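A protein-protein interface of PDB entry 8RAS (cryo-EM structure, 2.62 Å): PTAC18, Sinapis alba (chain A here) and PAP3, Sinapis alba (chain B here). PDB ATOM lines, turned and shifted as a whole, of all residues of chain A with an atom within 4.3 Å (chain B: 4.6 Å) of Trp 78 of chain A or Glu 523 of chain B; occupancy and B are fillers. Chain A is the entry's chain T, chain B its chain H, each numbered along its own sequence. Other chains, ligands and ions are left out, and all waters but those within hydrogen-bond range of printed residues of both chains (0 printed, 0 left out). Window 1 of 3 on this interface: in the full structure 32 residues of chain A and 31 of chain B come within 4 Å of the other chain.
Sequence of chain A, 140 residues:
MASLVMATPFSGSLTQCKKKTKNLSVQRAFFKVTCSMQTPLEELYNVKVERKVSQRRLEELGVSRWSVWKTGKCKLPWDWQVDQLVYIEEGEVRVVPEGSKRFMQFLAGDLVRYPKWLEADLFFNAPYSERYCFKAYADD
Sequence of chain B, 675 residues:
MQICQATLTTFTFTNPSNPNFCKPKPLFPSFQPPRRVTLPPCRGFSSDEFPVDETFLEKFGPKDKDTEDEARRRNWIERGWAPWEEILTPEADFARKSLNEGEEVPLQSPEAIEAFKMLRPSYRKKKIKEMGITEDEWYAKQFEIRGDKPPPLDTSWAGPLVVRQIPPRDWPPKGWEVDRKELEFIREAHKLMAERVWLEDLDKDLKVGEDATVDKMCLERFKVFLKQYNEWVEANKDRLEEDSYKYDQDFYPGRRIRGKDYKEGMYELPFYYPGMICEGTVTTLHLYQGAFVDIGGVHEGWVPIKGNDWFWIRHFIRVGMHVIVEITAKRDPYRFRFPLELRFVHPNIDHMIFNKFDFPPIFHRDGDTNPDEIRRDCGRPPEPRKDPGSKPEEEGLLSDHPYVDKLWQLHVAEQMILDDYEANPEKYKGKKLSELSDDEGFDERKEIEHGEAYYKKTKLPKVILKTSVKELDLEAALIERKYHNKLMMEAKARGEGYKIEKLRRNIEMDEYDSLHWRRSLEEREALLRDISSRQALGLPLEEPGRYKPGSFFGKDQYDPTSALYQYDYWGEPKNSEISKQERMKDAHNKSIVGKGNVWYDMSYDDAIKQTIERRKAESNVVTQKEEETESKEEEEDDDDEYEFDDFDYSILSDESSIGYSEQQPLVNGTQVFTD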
ATOM      1  N   LEU A  76       1.351 -13.765 -14.417  1.00  0.00           N
ATOM      2  CA  LEU A  76       1.680 -12.473 -15.010  1.00  0.00           C
ATOM      3  C   LEU A  76       3.088 -12.497 -15.586  1.00  0.00           C
ATOM      4  O   LEU A  76       4.062 -12.590 -14.822  1.00  0.00           O
ATOM      5  CB  LEU A  76       1.551 -11.358 -13.971  1.00  0.00           C
ATOM      6  CG  LEU A  76       2.132  -9.997 -14.361  1.00  0.00           C
ATOM      7  CD1 LEU A  76       1.424  -9.437 -15.585  1.00  0.00           C
ATOM      8  CD2 LEU A  76       2.050  -9.020 -13.200  1.00  0.00           C
ATOM      9  N   PRO A  77       3.253 -12.425 -16.907  1.00  0.00           N
ATOM     10  CA  PRO A  77       4.590 -12.280 -17.494  1.00  0.00           C
ATOM     11  C   PRO A  77       5.011 -10.819 -17.495  1.00  0.00           C
ATOM     12  O   PRO A  77       4.430  -9.989 -18.201  1.00  0.00           O
ATOM     13  CB  PRO A  77       4.407 -12.829 -18.917  1.00  0.00           C
ATOM     14  CG  PRO A  77       2.910 -13.017 -19.115  1.00  0.00           C
ATOM     15  CD  PRO A  77       2.202 -12.441 -17.933  1.00  0.00           C
ATOM     16  N   TRP A  78       6.029 -10.499 -16.701  1.00  0.00           N
ATOM     17  CA  TRP A  78       6.461  -9.125 -16.510  1.00  0.00           C
ATOM     18  C   TRP A  78       7.971  -9.026 -16.662  1.00  0.00           C
ATOM     19  O   TRP A  78       8.705  -9.979 -16.391  1.00  0.00           O
ATOM     20  CB  TRP A  78       6.047  -8.598 -15.128  1.00  0.00           C
ATOM     21  CG  TRP A  78       6.079  -7.109 -15.024  1.00  0.00           C
ATOM     22  CD1 TRP A  78       7.019  -6.351 -14.392  1.00  0.00           C
ATOM     23  CD2 TRP A  78       5.120  -6.192 -15.564  1.00  0.00           C
ATOM     24  NE1 TRP A  78       6.710  -5.018 -14.509  1.00  0.00           N
ATOM     25  CE2 TRP A  78       5.547  -4.894 -15.223  1.00  0.00           C
ATOM     26  CE3 TRP A  78       3.943  -6.341 -16.302  1.00  0.00           C
ATOM     27  CZ2 TRP A  78       4.839  -3.754 -15.595  1.00  0.00           C
ATOM     28  CZ3 TRP A  78       3.242  -5.209 -16.671  1.00  0.00           C
ATOM     29  CH2 TRP A  78       3.692  -3.932 -16.319  1.00  0.00           C
ATOM     30  N   ASP A  79       8.427  -7.855 -17.103  1.00  0.00           N
ATOM     31  CA  ASP A  79       9.845  -7.524 -17.156  1.00  0.00           C
ATOM     32  C   ASP A  79      10.076  -6.280 -16.311  1.00  0.00           C
ATOM     33  O   ASP A  79       9.479  -5.229 -16.571  1.00  0.00           O
ATOM     34  CB  ASP A  79      10.314  -7.303 -18.597  1.00  0.00           C
ATOM     35  CG  ASP A  79       9.463  -6.296 -19.343  1.00  0.00           C
ATOM     36  OD1 ASP A  79       8.235  -6.274 -19.121  1.00  0.00           O
ATOM     37  OD2 ASP A  79      10.021  -5.527 -20.153  1.00  0.00           O
ATOM     38  N   TRP A  80      10.932  -6.400 -15.299  1.00  0.00           N
ATOM     39  CA  TRP A  80      11.189  -5.302 -14.370  1.00  0.00           C
ATOM     40  C   TRP A  80      12.234  -4.381 -14.975  1.00  0.00           C
ATOM     41  O   TRP A  80      13.434  -4.546 -14.765  1.00  0.00           O
ATOM     42  CB  TRP A  80      11.657  -5.829 -13.022  1.00  0.00           C
ATOM     43  CG  TRP A  80      10.570  -6.395 -12.195  1.00  0.00           C
ATOM     44  CD1 TRP A  80       9.918  -5.789 -11.164  1.00  0.00           C
ATOM     45  CD2 TRP A  80       9.994  -7.692 -12.332  1.00  0.00           C
ATOM     46  NE1 TRP A  80       8.971  -6.638 -10.645  1.00  0.00           N
ATOM     47  CE2 TRP A  80       8.998  -7.813 -11.347  1.00  0.00           C
ATOM     48  CE3 TRP A  80      10.227  -8.768 -13.192  1.00  0.00           C
ATOM     49  CZ2 TRP A  80       8.237  -8.965 -11.200  1.00  0.00           C
ATOM     50  CZ3 TRP A  80       9.471  -9.906 -13.046  1.00  0.00           C
ATOM     51  CH2 TRP A  80       8.488  -9.997 -12.059  1.00  0.00           C
ATOM     52  N   GLN A  81      11.778  -3.388 -15.727  1.00  0.00           N
ATOM     53  CA  GLN A  81      12.680  -2.341 -16.184  1.00  0.00           C
ATOM     54  C   GLN A  81      12.830  -1.221 -15.165  1.00  0.00           C
ATOM     55  O   GLN A  81      13.516  -0.232 -15.447  1.00  0.00           O
ATOM     56  CB  GLN A  81      12.209  -1.798 -17.536  1.00  0.00           C
ATOM     57  CG  GLN A  81      10.794  -1.267 -17.546  1.00  0.00           C
ATOM     58  CD  GLN A  81      10.093  -1.531 -18.868  1.00  0.00           C
ATOM     59  OE1 GLN A  81      10.396  -2.504 -19.557  1.00  0.00           O
ATOM     60  NE2 GLN A  81       9.154  -0.664 -19.225  1.00  0.00           N
ATOM     61  N   VAL A  82      12.200  -1.351 -13.997  1.00  0.00           N
ATOM     62  CA  VAL A  82      12.427  -0.482 -12.852  1.00  0.00           C
ATOM     63  C   VAL A  82      12.561  -1.359 -11.614  1.00  0.00           C
ATOM     64  O   VAL A  82      11.970  -2.441 -11.533  1.00  0.00           O
ATOM     65  CB  VAL A  82      11.290   0.552 -12.660  1.00  0.00           C
ATOM     66  CG1 VAL A  82      11.703   1.625 -11.670  1.00  0.00           C
ATOM     67  CG2 VAL A  82      10.890   1.181 -13.988  1.00  0.00           C
ATOM     68  N   LEU A 118      15.016  -7.510 -14.917  1.00  0.00           N
ATOM     69  CA  LEU A 118      14.707  -8.906 -14.641  1.00  0.00           C
ATOM     70  C   LEU A 118      13.592  -9.392 -15.558  1.00  0.00           C
ATOM     71  O   LEU A 118      12.549  -8.744 -15.685  1.00  0.00           O
ATOM     72  CB  LEU A 118      14.305  -9.085 -13.179  1.00  0.00           C
ATOM     73  CG  LEU A 118      13.774 -10.469 -12.800  1.00  0.00           C
ATOM     74  CD1 LEU A 118      14.834 -11.534 -13.028  1.00  0.00           C
ATOM     75  CD2 LEU A 118      13.290 -10.490 -11.359  1.00  0.00           C
ATOM     76  N   ALA A 120      11.316 -12.248 -15.534  1.00  0.00           N
ATOM     77  CA  ALA A 120      10.763 -13.333 -14.738  1.00  0.00           C
ATOM     78  C   ALA A 120       9.300 -13.547 -15.121  1.00  0.00           C
ATOM     79  O   ALA A 120       8.782 -12.927 -16.054  1.00  0.00           O
ATOM     80  CB  ALA A 120      10.932 -13.041 -13.247  1.00  0.00           C
ATOM     81  N   PHE A 134       7.945   1.187  -6.210  1.00  0.00           N
ATOM     82  CA  PHE A 134       8.796   1.356  -7.381  1.00  0.00           C
ATOM     83  C   PHE A 134       9.802   2.464  -7.111  1.00  0.00           C
ATOM     84  O   PHE A 134       9.426   3.576  -6.725  1.00  0.00           O
ATOM     85  CB  PHE A 134       7.961   1.683  -8.620  1.00  0.00           C
ATOM     86  CG  PHE A 134       7.213   0.506  -9.180  1.00  0.00           C
ATOM     87  CD1 PHE A 134       7.890  -0.526  -9.802  1.00  0.00           C
ATOM     88  CD2 PHE A 134       5.837   0.427  -9.072  1.00  0.00           C
ATOM     89  CE1 PHE A 134       7.210  -1.611 -10.312  1.00  0.00           C
ATOM     90  CE2 PHE A 134       5.148  -0.658  -9.581  1.00  0.00           C
ATOM     91  CZ  PHE A 134       5.838  -1.678 -10.203  1.00  0.00           C
ATOM     92  N   LEU B 398      -0.418  -0.504 -19.383  1.00  0.00           N
ATOM     93  CA  LEU B 398      -1.075  -1.804 -19.396  1.00  0.00           C
ATOM     94  C   LEU B 398      -2.114  -1.861 -18.286  1.00  0.00           C
ATOM     95  O   LEU B 398      -1.814  -1.535 -17.132  1.00  0.00           O
ATOM     96  CB  LEU B 398      -0.052  -2.928 -19.222  1.00  0.00           C
ATOM     97  CG  LEU B 398       0.968  -3.138 -20.344  1.00  0.00           C
ATOM     98  CD1 LEU B 398       1.394  -4.592 -20.400  1.00  0.00           C
ATOM     99  CD2 LEU B 398       0.414  -2.693 -21.691  1.00  0.00           C
ATOM    100  N   ARG B 519      -0.691   0.194 -11.369  1.00  0.00           N
ATOM    101  CA  ARG B 519       0.587  -0.491 -11.490  1.00  0.00           C
ATOM    102  C   ARG B 519       1.392   0.147 -12.614  1.00  0.00           C
ATOM    103  O   ARG B 519       2.544   0.571 -12.435  1.00  0.00           O
ATOM    104  CB  ARG B 519       0.341  -1.976 -11.806  1.00  0.00           C
ATOM    105  CG  ARG B 519       0.365  -2.964 -10.654  1.00  0.00           C
ATOM    106  CD  ARG B 519       1.424  -2.630  -9.695  1.00  0.00           C
ATOM    107  NE  ARG B 519       1.262  -3.296  -8.412  1.00  0.00           N
ATOM    108  CZ  ARG B 519       1.841  -2.852  -7.310  1.00  0.00           C
ATOM    109  NH1 ARG B 519       2.534  -1.733  -7.312  1.00  0.00           N
ATOM    110  NH2 ARG B 519       1.750  -3.562  -6.191  1.00  0.00           N
ATOM    111  N   SER B 520       0.745   0.251 -13.778  1.00  0.00           N
ATOM    112  CA  SER B 520       1.380   0.824 -14.956  1.00  0.00           C
ATOM    113  C   SER B 520       1.809   2.269 -14.718  1.00  0.00           C
ATOM    114  O   SER B 520       2.919   2.660 -15.090  1.00  0.00           O
ATOM    115  CB  SER B 520       0.424   0.741 -16.142  1.00  0.00           C
ATOM    116  OG  SER B 520       0.231  -0.603 -16.541  1.00  0.00           O
ATOM    117  N   LEU B 521       0.936   3.091 -14.117  1.00  0.00           N
ATOM    118  CA  LEU B 521       1.304   4.502 -13.989  1.00  0.00           C
ATOM    119  C   LEU B 521       2.495   4.671 -13.056  1.00  0.00           C
ATOM    120  O   LEU B 521       3.420   5.434 -13.353  1.00  0.00           O
ATOM    121  CB  LEU B 521       0.164   5.390 -13.481  1.00  0.00           C
ATOM    122  CG  LEU B 521      -0.568   5.195 -12.159  1.00  0.00           C
ATOM    123  CD1 LEU B 521      -0.095   6.256 -11.189  1.00  0.00           C
ATOM    124  CD2 LEU B 521      -2.024   5.422 -12.379  1.00  0.00           C
ATOM    125  N   GLU B 522       2.478   3.994 -11.902  1.00  0.00           N
ATOM    126  CA  GLU B 522       3.577   4.181 -10.960  1.00  0.00           C
ATOM    127  C   GLU B 522       4.883   3.642 -11.525  1.00  0.00           C
ATOM    128  O   GLU B 522       5.944   4.271 -11.366  1.00  0.00           O
ATOM    129  CB  GLU B 522       3.249   3.542  -9.608  1.00  0.00           C
ATOM    130  CG  GLU B 522       2.900   2.073  -9.644  1.00  0.00           C
ATOM    131  CD  GLU B 522       1.757   1.737  -8.706  1.00  0.00           C
ATOM    132  OE1 GLU B 522       1.105   2.676  -8.204  1.00  0.00           O
ATOM    133  OE2 GLU B 522       1.503   0.538  -8.475  1.00  0.00           O
ATOM    134  N   GLU B 523       4.831   2.497 -12.216  1.00  0.00           N
ATOM    135  CA  GLU B 523       6.039   1.994 -12.856  1.00  0.00           C
ATOM    136  C   GLU B 523       6.532   2.964 -13.923  1.00  0.00           C
ATOM    137  O   GLU B 523       7.738   3.191 -14.051  1.00  0.00           O
ATOM    138  CB  GLU B 523       5.791   0.608 -13.448  1.00  0.00           C
ATOM    139  CG  GLU B 523       7.018   0.009 -14.119  1.00  0.00           C
ATOM    140  CD  GLU B 523       6.953  -1.501 -14.232  1.00  0.00           C
ATOM    141  OE1 GLU B 523       6.436  -2.149 -13.299  1.00  0.00           O
ATOM    142  OE2 GLU B 523       7.439  -2.043 -15.244  1.00  0.00           O
ATOM    143  N   ARG B 524       5.611   3.575 -14.674  1.00  0.00           N
ATOM    144  CA  ARG B 524       6.003   4.529 -15.708  1.00  0.00           C
ATOM    145  C   ARG B 524       6.639   5.779 -15.112  1.00  0.00           C
ATOM    146  O   ARG B 524       7.607   6.309 -15.665  1.00  0.00           O
ATOM    147  CB  ARG B 524       4.790   4.907 -16.557  1.00  0.00           C
ATOM    148  CG  ARG B 524       5.132   5.673 -17.821  1.00  0.00           C
ATOM    149  CD  ARG B 524       5.981   4.830 -18.754  1.00  0.00           C
ATOM    150  NE  ARG B 524       5.412   3.502 -18.951  1.00  0.00           N
ATOM    151  CZ  ARG B 524       4.871   3.080 -20.085  1.00  0.00           C
ATOM    152  NH1 ARG B 524       4.811   3.856 -21.154  1.00  0.00           N
ATOM    153  NH2 ARG B 524       4.376   1.847 -20.149  1.00  0.00           N
ATOM    154  N   GLU B 525       6.097   6.284 -14.002  1.00  0.00           N
ATOM    155  CA  GLU B 525       6.680   7.477 -13.390  1.00  0.00           C
ATOM    156  C   GLU B 525       8.067   7.186 -12.833  1.00  0.00           C
ATOM    157  O   GLU B 525       9.004   7.976 -13.032  1.00  0.00           O
ATOM    158  CB  GLU B 525       5.765   8.026 -12.294  1.00  0.00           C
ATOM    159  CG  GLU B 525       4.643   8.915 -12.812  1.00  0.00           C
ATOM    160  CD  GLU B 525       3.281   8.265 -12.719  1.00  0.00           C
ATOM    161  OE1 GLU B 525       2.984   7.649 -11.674  1.00  0.00           O
ATOM    162  OE2 GLU B 525       2.509   8.359 -13.695  1.00  0.00           O
ATOM    163  N   ALA B 526       8.221   6.055 -12.138  1.00  0.00           N
ATOM    164  CA  ALA B 526       9.555   5.644 -11.715  1.00  0.00           C
ATOM    165  C   ALA B 526      10.478   5.501 -12.919  1.00  0.00           C
ATOM    166  O   ALA B 526      11.663   5.845 -12.853  1.00  0.00           O
ATOM    167  CB  ALA B 526       9.476   4.338 -10.928  1.00  0.00           C
ATOM    168  N   LEU B 527       9.934   5.027 -14.041  1.00  0.00           N
ATOM    169  CA  LEU B 527      10.723   4.852 -15.252  1.00  0.00           C
ATOM    170  C   LEU B 527      11.228   6.186 -15.786  1.00  0.00           C
ATOM    171  O   LEU B 527      12.417   6.328 -16.087  1.00  0.00           O
ATOM    172  CB  LEU B 527       9.873   4.126 -16.294  1.00  0.00           C
ATOM    173  CG  LEU B 527      10.517   3.374 -17.450  1.00  0.00           C
ATOM    174  CD1 LEU B 527       9.836   2.041 -17.553  1.00  0.00           C
ATOM    175  CD2 LEU B 527      10.339   4.124 -18.744  1.00  0.00           C
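Gln 81 of chain A touches Leu 527 of chain B (NE2 to CD1, 3.3 Å). O of Glu 523 of chain B touches CG2 of Val 82 of chain A (3.7 Å). Val 82 of chain A touches Ala 526 of chain B (CG1 to CB, 3.6 Å). Val 82 of chain A touches Leu 527 of chain B (CG2 to CD1, 3.8 Å). NH1 of Arg 519 of chain B touches CE2 of Phe 134 of chain A, 3.6 Å away. Phe 134 of chain A touches Glu 522 of chain B (CD2 to CG, 3.4 Å). Phe 134 of chain A touches Glu 523 of chain B. Ala 526 of chain B touches Phe 134 of chain A.
NE1 of Trp 78 of chain A lies within hydrogen-bond range of OE1 of Glu 523 of chain B.
Trp 78 of chain A touches one residue of chain B. Trp 80 of chain A touches none of the printed residues of chain B. Of the printed residues of chain B, Val 82 of chain A touches Glu 523, Ala 526 and Leu 527. Of the printed residues of chain A, Arg 519 of chain B touches Phe 134. Ser 520 of chain B touches none of the printed residues of chain A. Of the printed residues of chain A, Glu 523 of chain B touches Trp 78, Val 82 and Phe 134. The nearest printed residue of chain A that does not touch Glu 523 of chain B is Asp 79 of chain A (4.01 Å).
Among the printed residues, 9 pairs touch across the chains.
The side-chain carboxylate (OE2) of Glu 522 of chain B lies within salt-bridge range of the guanidinium group (NH1) of Arg 519 of chain B. The side-chain amide oxygen (OE1) of Gln 81 of chain A sits close to the side-chain carboxylate (OD2) of Asp 79 of chain A (3.1 Å).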
